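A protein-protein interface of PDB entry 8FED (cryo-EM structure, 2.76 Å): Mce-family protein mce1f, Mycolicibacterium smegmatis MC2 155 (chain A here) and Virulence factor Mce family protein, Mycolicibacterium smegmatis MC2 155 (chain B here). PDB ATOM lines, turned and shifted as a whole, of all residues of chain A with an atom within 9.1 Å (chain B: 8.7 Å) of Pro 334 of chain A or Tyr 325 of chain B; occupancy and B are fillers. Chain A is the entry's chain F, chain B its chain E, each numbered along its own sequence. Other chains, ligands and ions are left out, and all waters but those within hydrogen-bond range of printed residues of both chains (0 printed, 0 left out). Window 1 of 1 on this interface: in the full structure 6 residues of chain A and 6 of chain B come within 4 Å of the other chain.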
ATOM      1  N   ALA A 328     -23.971  18.022 -19.913  1.00  0.00           N
ATOM      2  CA  ALA A 328     -23.759  16.657 -20.378  1.00  0.00           C
ATOM      3  C   ALA A 328     -22.296  16.238 -20.315  1.00  0.00           C
ATOM      4  O   ALA A 328     -22.012  15.038 -20.245  1.00  0.00           O
ATOM      5  CB  ALA A 328     -24.287  16.502 -21.805  1.00  0.00           C
ATOM      6  N   GLN A 330     -20.338  17.174 -17.817  1.00  0.00           N
ATOM      7  CA  GLN A 330     -20.009  17.103 -16.400  1.00  0.00           C
ATOM      8  C   GLN A 330     -20.446  15.794 -15.753  1.00  0.00           C
ATOM      9  O   GLN A 330     -20.260  15.629 -14.544  1.00  0.00           O
ATOM     10  CB  GLN A 330     -20.641  18.279 -15.649  1.00  0.00           C
ATOM     11  CG  GLN A 330     -20.152  19.649 -16.099  1.00  0.00           C
ATOM     12  CD  GLN A 330     -18.683  19.880 -15.802  1.00  0.00           C
ATOM     13  OE1 GLN A 330     -18.129  19.311 -14.862  1.00  0.00           O
ATOM     14  NE2 GLN A 330     -18.044  20.721 -16.605  1.00  0.00           N
ATOM     15  N   TRP A 331     -21.030  14.876 -16.520  1.00  0.00           N
ATOM     16  CA  TRP A 331     -21.407  13.576 -15.981  1.00  0.00           C
ATOM     17  C   TRP A 331     -20.160  12.777 -15.621  1.00  0.00           C
ATOM     18  O   TRP A 331     -19.185  12.745 -16.376  1.00  0.00           O
ATOM     19  CB  TRP A 331     -22.259  12.803 -16.990  1.00  0.00           C
ATOM     20  CG  TRP A 331     -23.609  13.414 -17.269  1.00  0.00           C
ATOM     21  CD1 TRP A 331     -24.068  14.628 -16.843  1.00  0.00           C
ATOM     22  CD2 TRP A 331     -24.670  12.833 -18.036  1.00  0.00           C
ATOM     23  NE1 TRP A 331     -25.347  14.837 -17.297  1.00  0.00           N
ATOM     24  CE2 TRP A 331     -25.740  13.751 -18.032  1.00  0.00           C
ATOM     25  CE3 TRP A 331     -24.820  11.627 -18.725  1.00  0.00           C
ATOM     26  CZ2 TRP A 331     -26.941  13.499 -18.690  1.00  0.00           C
ATOM     27  CZ3 TRP A 331     -26.014  11.379 -19.378  1.00  0.00           C
ATOM     28  CH2 TRP A 331     -27.059  12.311 -19.356  1.00  0.00           C
ATOM     29  N   ARG A 332     -20.195  12.131 -14.460  1.00  0.00           N
ATOM     30  CA  ARG A 332     -19.037  11.431 -13.928  1.00  0.00           C
ATOM     31  C   ARG A 332     -19.090   9.948 -14.273  1.00  0.00           C
ATOM     32  O   ARG A 332     -20.164   9.351 -14.380  1.00  0.00           O
ATOM     33  CB  ARG A 332     -18.946  11.603 -12.410  1.00  0.00           C
ATOM     34  CG  ARG A 332     -19.088  13.039 -11.936  1.00  0.00           C
ATOM     35  CD  ARG A 332     -18.506  13.255 -10.544  1.00  0.00           C
ATOM     36  NE  ARG A 332     -19.018  12.311  -9.557  1.00  0.00           N
ATOM     37  CZ  ARG A 332     -18.326  11.293  -9.063  1.00  0.00           C
ATOM     38  NH1 ARG A 332     -17.082  11.054  -9.443  1.00  0.00           N
ATOM     39  NH2 ARG A 332     -18.895  10.497  -8.163  1.00  0.00           N
ATOM     40  N   SER A 333     -17.909   9.363 -14.447  1.00  0.00           N
ATOM     41  CA  SER A 333     -17.810   7.952 -14.772  1.00  0.00           C
ATOM     42  C   SER A 333     -18.254   7.103 -13.581  1.00  0.00           C
ATOM     43  O   SER A 333     -18.038   7.480 -12.427  1.00  0.00           O
ATOM     44  CB  SER A 333     -16.375   7.599 -15.160  1.00  0.00           C
ATOM     45  OG  SER A 333     -16.233   6.213 -15.410  1.00  0.00           O
ATOM     46  N   PRO A 334     -18.891   5.956 -13.835  1.00  0.00           N
ATOM     47  CA  PRO A 334     -19.296   5.080 -12.724  1.00  0.00           C
ATOM     48  C   PRO A 334     -18.135   4.405 -12.016  1.00  0.00           C
ATOM     49  O   PRO A 334     -18.332   3.877 -10.915  1.00  0.00           O
ATOM     50  CB  PRO A 334     -20.205   4.050 -13.405  1.00  0.00           C
ATOM     51  CG  PRO A 334     -19.750   4.027 -14.821  1.00  0.00           C
ATOM     52  CD  PRO A 334     -19.331   5.433 -15.140  1.00  0.00           C
ATOM     53  N   ALA A 335     -16.936   4.403 -12.604  1.00  0.00           N
ATOM     54  CA  ALA A 335     -15.790   3.746 -11.990  1.00  0.00           C
ATOM     55  C   ALA A 335     -15.274   4.478 -10.757  1.00  0.00           C
ATOM     56  O   ALA A 335     -14.462   3.909 -10.020  1.00  0.00           O
ATOM     57  CB  ALA A 335     -14.663   3.602 -13.013  1.00  0.00           C
ATOM     58  N   ASP A 336     -15.716   5.710 -10.518  1.00  0.00           N
ATOM     59  CA  ASP A 336     -15.266   6.513  -9.388  1.00  0.00           C
ATOM     60  C   ASP A 336     -16.371   6.559  -8.343  1.00  0.00           C
ATOM     61  O   ASP A 336     -17.483   7.015  -8.630  1.00  0.00           O
ATOM     62  CB  ASP A 336     -14.888   7.924  -9.837  1.00  0.00           C
ATOM     63  CG  ASP A 336     -13.838   7.924 -10.929  1.00  0.00           C
ATOM     64  OD1 ASP A 336     -12.990   7.007 -10.939  1.00  0.00           O
ATOM     65  OD2 ASP A 336     -13.860   8.838 -11.780  1.00  0.00           O
ATOM     66  N   THR A 337     -16.060   6.094  -7.135  1.00  0.00           N
ATOM     67  CA  THR A 337     -17.006   6.071  -6.029  1.00  0.00           C
ATOM     68  C   THR A 337     -16.885   7.284  -5.116  1.00  0.00           C
ATOM     69  O   THR A 337     -17.608   7.365  -4.118  1.00  0.00           O
ATOM     70  CB  THR A 337     -16.824   4.792  -5.206  1.00  0.00           C
ATOM     71  OG1 THR A 337     -15.485   4.737  -4.702  1.00  0.00           O
ATOM     72  CG2 THR A 337     -17.083   3.567  -6.066  1.00  0.00           C
ATOM     73  N   ARG A 338     -15.992   8.220  -5.427  1.00  0.00           N
ATOM     74  CA  ARG A 338     -15.816   9.404  -4.598  1.00  0.00           C
ATOM     75  C   ARG A 338     -17.031  10.317  -4.698  1.00  0.00           C
ATOM     76  O   ARG A 338     -17.496  10.636  -5.797  1.00  0.00           O
ATOM     77  CB  ARG A 338     -14.551  10.150  -5.022  1.00  0.00           C
ATOM     78  CG  ARG A 338     -14.513  11.616  -4.631  1.00  0.00           C
ATOM     79  CD  ARG A 338     -13.164  12.224  -4.975  1.00  0.00           C
ATOM     80  NE  ARG A 338     -12.673  11.747  -6.263  1.00  0.00           N
ATOM     81  CZ  ARG A 338     -11.466  12.005  -6.748  1.00  0.00           C
ATOM     82  NH1 ARG A 338     -10.597  12.746  -6.081  1.00  0.00           N
ATOM     83  NH2 ARG A 338     -11.124  11.507  -7.933  1.00  0.00           N
ATOM     84  N   THR A 339     -17.544  10.742  -3.545  1.00  0.00           N
ATOM     85  CA  THR A 339     -18.723  11.594  -3.483  1.00  0.00           C
ATOM     86  C   THR A 339     -18.300  13.057  -3.493  1.00  0.00           C
ATOM     87  O   THR A 339     -17.391  13.454  -2.757  1.00  0.00           O
ATOM     88  CB  THR A 339     -19.548  11.283  -2.232  1.00  0.00           C
ATOM     89  OG1 THR A 339     -19.933   9.903  -2.246  1.00  0.00           O
ATOM     90  CG2 THR A 339     -20.800  12.147  -2.183  1.00  0.00           C
ATOM     91  N   ILE B 317     -27.547   3.126   3.152  1.00  0.00           N
ATOM     92  CA  ILE B 317     -27.324   4.068   2.049  1.00  0.00           C
ATOM     93  C   ILE B 317     -25.857   4.164   1.635  1.00  0.00           C
ATOM     94  O   ILE B 317     -25.583   4.133   0.425  1.00  0.00           O
ATOM     95  CB  ILE B 317     -27.923   5.442   2.397  1.00  0.00           C
ATOM     96  CG1 ILE B 317     -29.436   5.346   2.554  1.00  0.00           C
ATOM     97  CG2 ILE B 317     -27.582   6.460   1.328  1.00  0.00           C
ATOM     98  CD1 ILE B 317     -30.149   4.936   1.296  1.00  0.00           C
ATOM     99  N   LYS B 319     -23.487   2.183   1.295  1.00  0.00           N
ATOM    100  CA  LYS B 319     -22.965   1.069   0.513  1.00  0.00           C
ATOM    101  C   LYS B 319     -23.826   0.707  -0.686  1.00  0.00           C
ATOM    102  O   LYS B 319     -23.305   0.138  -1.647  1.00  0.00           O
ATOM    103  CB  LYS B 319     -22.790  -0.172   1.398  1.00  0.00           C
ATOM    104  CG  LYS B 319     -24.051  -0.652   2.097  1.00  0.00           C
ATOM    105  CD  LYS B 319     -23.725  -1.792   3.049  1.00  0.00           C
ATOM    106  CE  LYS B 319     -24.976  -2.435   3.612  1.00  0.00           C
ATOM    107  NZ  LYS B 319     -24.651  -3.543   4.552  1.00  0.00           N
ATOM    108  N   ALA B 320     -25.124   1.011  -0.660  1.00  0.00           N
ATOM    109  CA  ALA B 320     -25.949   0.797  -1.843  1.00  0.00           C
ATOM    110  C   ALA B 320     -25.615   1.807  -2.935  1.00  0.00           C
ATOM    111  O   ALA B 320     -25.449   1.440  -4.104  1.00  0.00           O
ATOM    112  CB  ALA B 320     -27.432   0.877  -1.476  1.00  0.00           C
ATOM    113  N   ILE B 321     -25.502   3.079  -2.572  1.00  0.00           N
ATOM    114  CA  ILE B 321     -25.281   4.164  -3.522  1.00  0.00           C
ATOM    115  C   ILE B 321     -23.816   4.566  -3.433  1.00  0.00           C
ATOM    116  O   ILE B 321     -23.399   5.213  -2.467  1.00  0.00           O
ATOM    117  CB  ILE B 321     -26.205   5.354  -3.242  1.00  0.00           C
ATOM    118  CG1 ILE B 321     -27.648   4.884  -3.068  1.00  0.00           C
ATOM    119  CG2 ILE B 321     -26.110   6.367  -4.364  1.00  0.00           C
ATOM    120  CD1 ILE B 321     -28.629   6.006  -2.838  1.00  0.00           C
ATOM    121  N   ARG B 322     -23.031   4.192  -4.436  1.00  0.00           N
ATOM    122  CA  ARG B 322     -21.597   4.487  -4.454  1.00  0.00           C
ATOM    123  C   ARG B 322     -21.285   5.744  -5.256  1.00  0.00           C
ATOM    124  O   ARG B 322     -20.429   5.747  -6.139  1.00  0.00           O
ATOM    125  CB  ARG B 322     -20.832   3.292  -5.004  1.00  0.00           C
ATOM    126  CG  ARG B 322     -21.229   1.973  -4.377  1.00  0.00           C
ATOM    127  CD  ARG B 322     -20.775   1.877  -2.937  1.00  0.00           C
ATOM    128  NE  ARG B 322     -21.097   0.577  -2.364  1.00  0.00           N
ATOM    129  CZ  ARG B 322     -20.334  -0.500  -2.479  1.00  0.00           C
ATOM    130  NH1 ARG B 322     -19.190  -0.469  -3.142  1.00  0.00           N
ATOM    131  NH2 ARG B 322     -20.730  -1.639  -1.916  1.00  0.00           N
ATOM    132  N   GLY B 323     -21.975   6.838  -4.943  1.00  0.00           N
ATOM    133  CA  GLY B 323     -21.738   8.100  -5.614  1.00  0.00           C
ATOM    134  C   GLY B 323     -22.891   8.586  -6.466  1.00  0.00           C
ATOM    135  O   GLY B 323     -23.963   8.907  -5.945  1.00  0.00           O
ATOM    136  N   ASP B 324     -22.682   8.648  -7.778  1.00  0.00           N
ATOM    137  CA  ASP B 324     -23.661   9.205  -8.703  1.00  0.00           C
ATOM    138  C   ASP B 324     -24.650   8.179  -9.239  1.00  0.00           C
ATOM    139  O   ASP B 324     -25.553   8.555  -9.993  1.00  0.00           O
ATOM    140  CB  ASP B 324     -22.947   9.880  -9.880  1.00  0.00           C
ATOM    141  CG  ASP B 324     -22.493  11.288  -9.559  1.00  0.00           C
ATOM    142  OD1 ASP B 324     -23.251  12.019  -8.893  1.00  0.00           O
ATOM    143  OD2 ASP B 324     -21.378  11.669  -9.974  1.00  0.00           O
ATOM    144  N   TYR B 325     -24.504   6.900  -8.896  1.00  0.00           N
ATOM    145  CA  TYR B 325     -25.352   5.848  -9.447  1.00  0.00           C
ATOM    146  C   TYR B 325     -25.869   4.952  -8.333  1.00  0.00           C
ATOM    147  O   TYR B 325     -25.077   4.366  -7.588  1.00  0.00           O
ATOM    148  CB  TYR B 325     -24.587   5.022 -10.483  1.00  0.00           C
ATOM    149  CG  TYR B 325     -24.084   5.834 -11.651  1.00  0.00           C
ATOM    150  CD1 TYR B 325     -24.955   6.280 -12.633  1.00  0.00           C
ATOM    151  CD2 TYR B 325     -22.742   6.154 -11.771  1.00  0.00           C
ATOM    152  CE1 TYR B 325     -24.503   7.023 -13.702  1.00  0.00           C
ATOM    153  CE2 TYR B 325     -22.281   6.897 -12.836  1.00  0.00           C
ATOM    154  CZ  TYR B 325     -23.163   7.328 -13.800  1.00  0.00           C
ATOM    155  OH  TYR B 325     -22.701   8.069 -14.863  1.00  0.00           O
ATOM    156  N   ILE B 326     -27.192   4.834  -8.230  1.00  0.00           N
ATOM    157  CA  ILE B 326     -27.792   3.873  -7.312  1.00  0.00           C
ATOM    158  C   ILE B 326     -27.577   2.471  -7.860  1.00  0.00           C
ATOM    159  O   ILE B 326     -27.904   2.185  -9.018  1.00  0.00           O
ATOM    160  CB  ILE B 326     -29.289   4.156  -7.128  1.00  0.00           C
ATOM    161  CG1 ILE B 326     -29.523   5.565  -6.590  1.00  0.00           C
ATOM    162  CG2 ILE B 326     -29.916   3.126  -6.207  1.00  0.00           C
ATOM    163  CD1 ILE B 326     -30.987   5.886  -6.369  1.00  0.00           C
ATOM    164  N   ASN B 327     -27.030   1.586  -7.034  1.00  0.00           N
ATOM    165  CA  ASN B 327     -26.916   0.192  -7.429  1.00  0.00           C
ATOM    166  C   ASN B 327     -28.271  -0.495  -7.343  1.00  0.00           C
ATOM    167  O   ASN B 327     -29.149  -0.091  -6.577  1.00  0.00           O
ATOM    168  CB  ASN B 327     -25.906  -0.537  -6.549  1.00  0.00           C
ATOM    169  CG  ASN B 327     -24.481  -0.223  -6.927  1.00  0.00           C
ATOM    170  OD1 ASN B 327     -24.215   0.748  -7.634  1.00  0.00           O
ATOM    171  ND2 ASN B 327     -23.551  -1.033  -6.448  1.00  0.00           N
ATOM    172  N   VAL B 328     -28.436  -1.544  -8.148  1.00  0.00           N
ATOM    173  CA  VAL B 328     -29.682  -2.298  -8.180  1.00  0.00           C
ATOM    174  C   VAL B 328     -29.393  -3.641  -8.829  1.00  0.00           C
ATOM    175  O   VAL B 328     -28.458  -3.776  -9.622  1.00  0.00           O
ATOM    176  CB  VAL B 328     -30.795  -1.510  -8.921  1.00  0.00           C
ATOM    177  CG1 VAL B 328     -30.537  -1.479 -10.418  1.00  0.00           C
ATOM    178  CG2 VAL B 328     -32.175  -2.071  -8.602  1.00  0.00           C
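Of the 11 printed residues of chain A, 3 touch a printed residue of chain B. Printed residues of chain A that touch a printed residue of chain B: Arg 332, Pro 334 and Thr 337. Among the printed residues, Asp or Glu carboxylates within 4 Å of a Lys or Arg side-chain nitrogen of the other chain: Arg 332 of chain A with Asp 324 of chain B (2.5 Å).
The guanidinium group (NH2) of Arg 332 of chain A lies within hydrogen-bond range of the backbone carbonyl oxygen (O) of Arg 338 of chain A, 2.8 Å away. The backbone carbonyl oxygen (O) of Lys 319 of chain B is in hydrogen-bond range of the guanidinium group (NH2) of Arg 322 of chain B.
Of the printed residues of chain B, Arg 332 of chain A touches Asp 324 (2.5 Å) and Tyr 325 (2.9 Å). No residue of chain B comes within 4 Å of Ser 333 of chain A. Printed residues of chain B within 4 Å of Thr 337 of chain A: Arg 322 (3.4 Å). Of the printed residues of chain A, Arg 322 of chain B touches Thr 337. Printed residues of chain A within 4 Å of Asp 324 of chain B: Arg 332 (2.5 Å). Of chain A, only Arg 332 and Pro 334 come within 4 Å of Tyr 325 of chain B. The nearest printed residue of chain A that does not touch Arg 322 of chain B is Asp 336 of chain A (4.1 Å).
CE2 of Tyr 325 of chain B touches CA of Pro 334 of chain A, at 3.5 Å. Thr 337 of chain A touches Arg 322 of chain B (CA to O, 3.4 Å).
OD2 of Asp 324 of chain B is in salt-bridge range of NE of Arg 332 of chain A. The side-chain hydroxyl of Tyr 325 of chain B is in hydrogen-bond range of the backbone carbonyl oxygen of Arg 332 of chain A.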
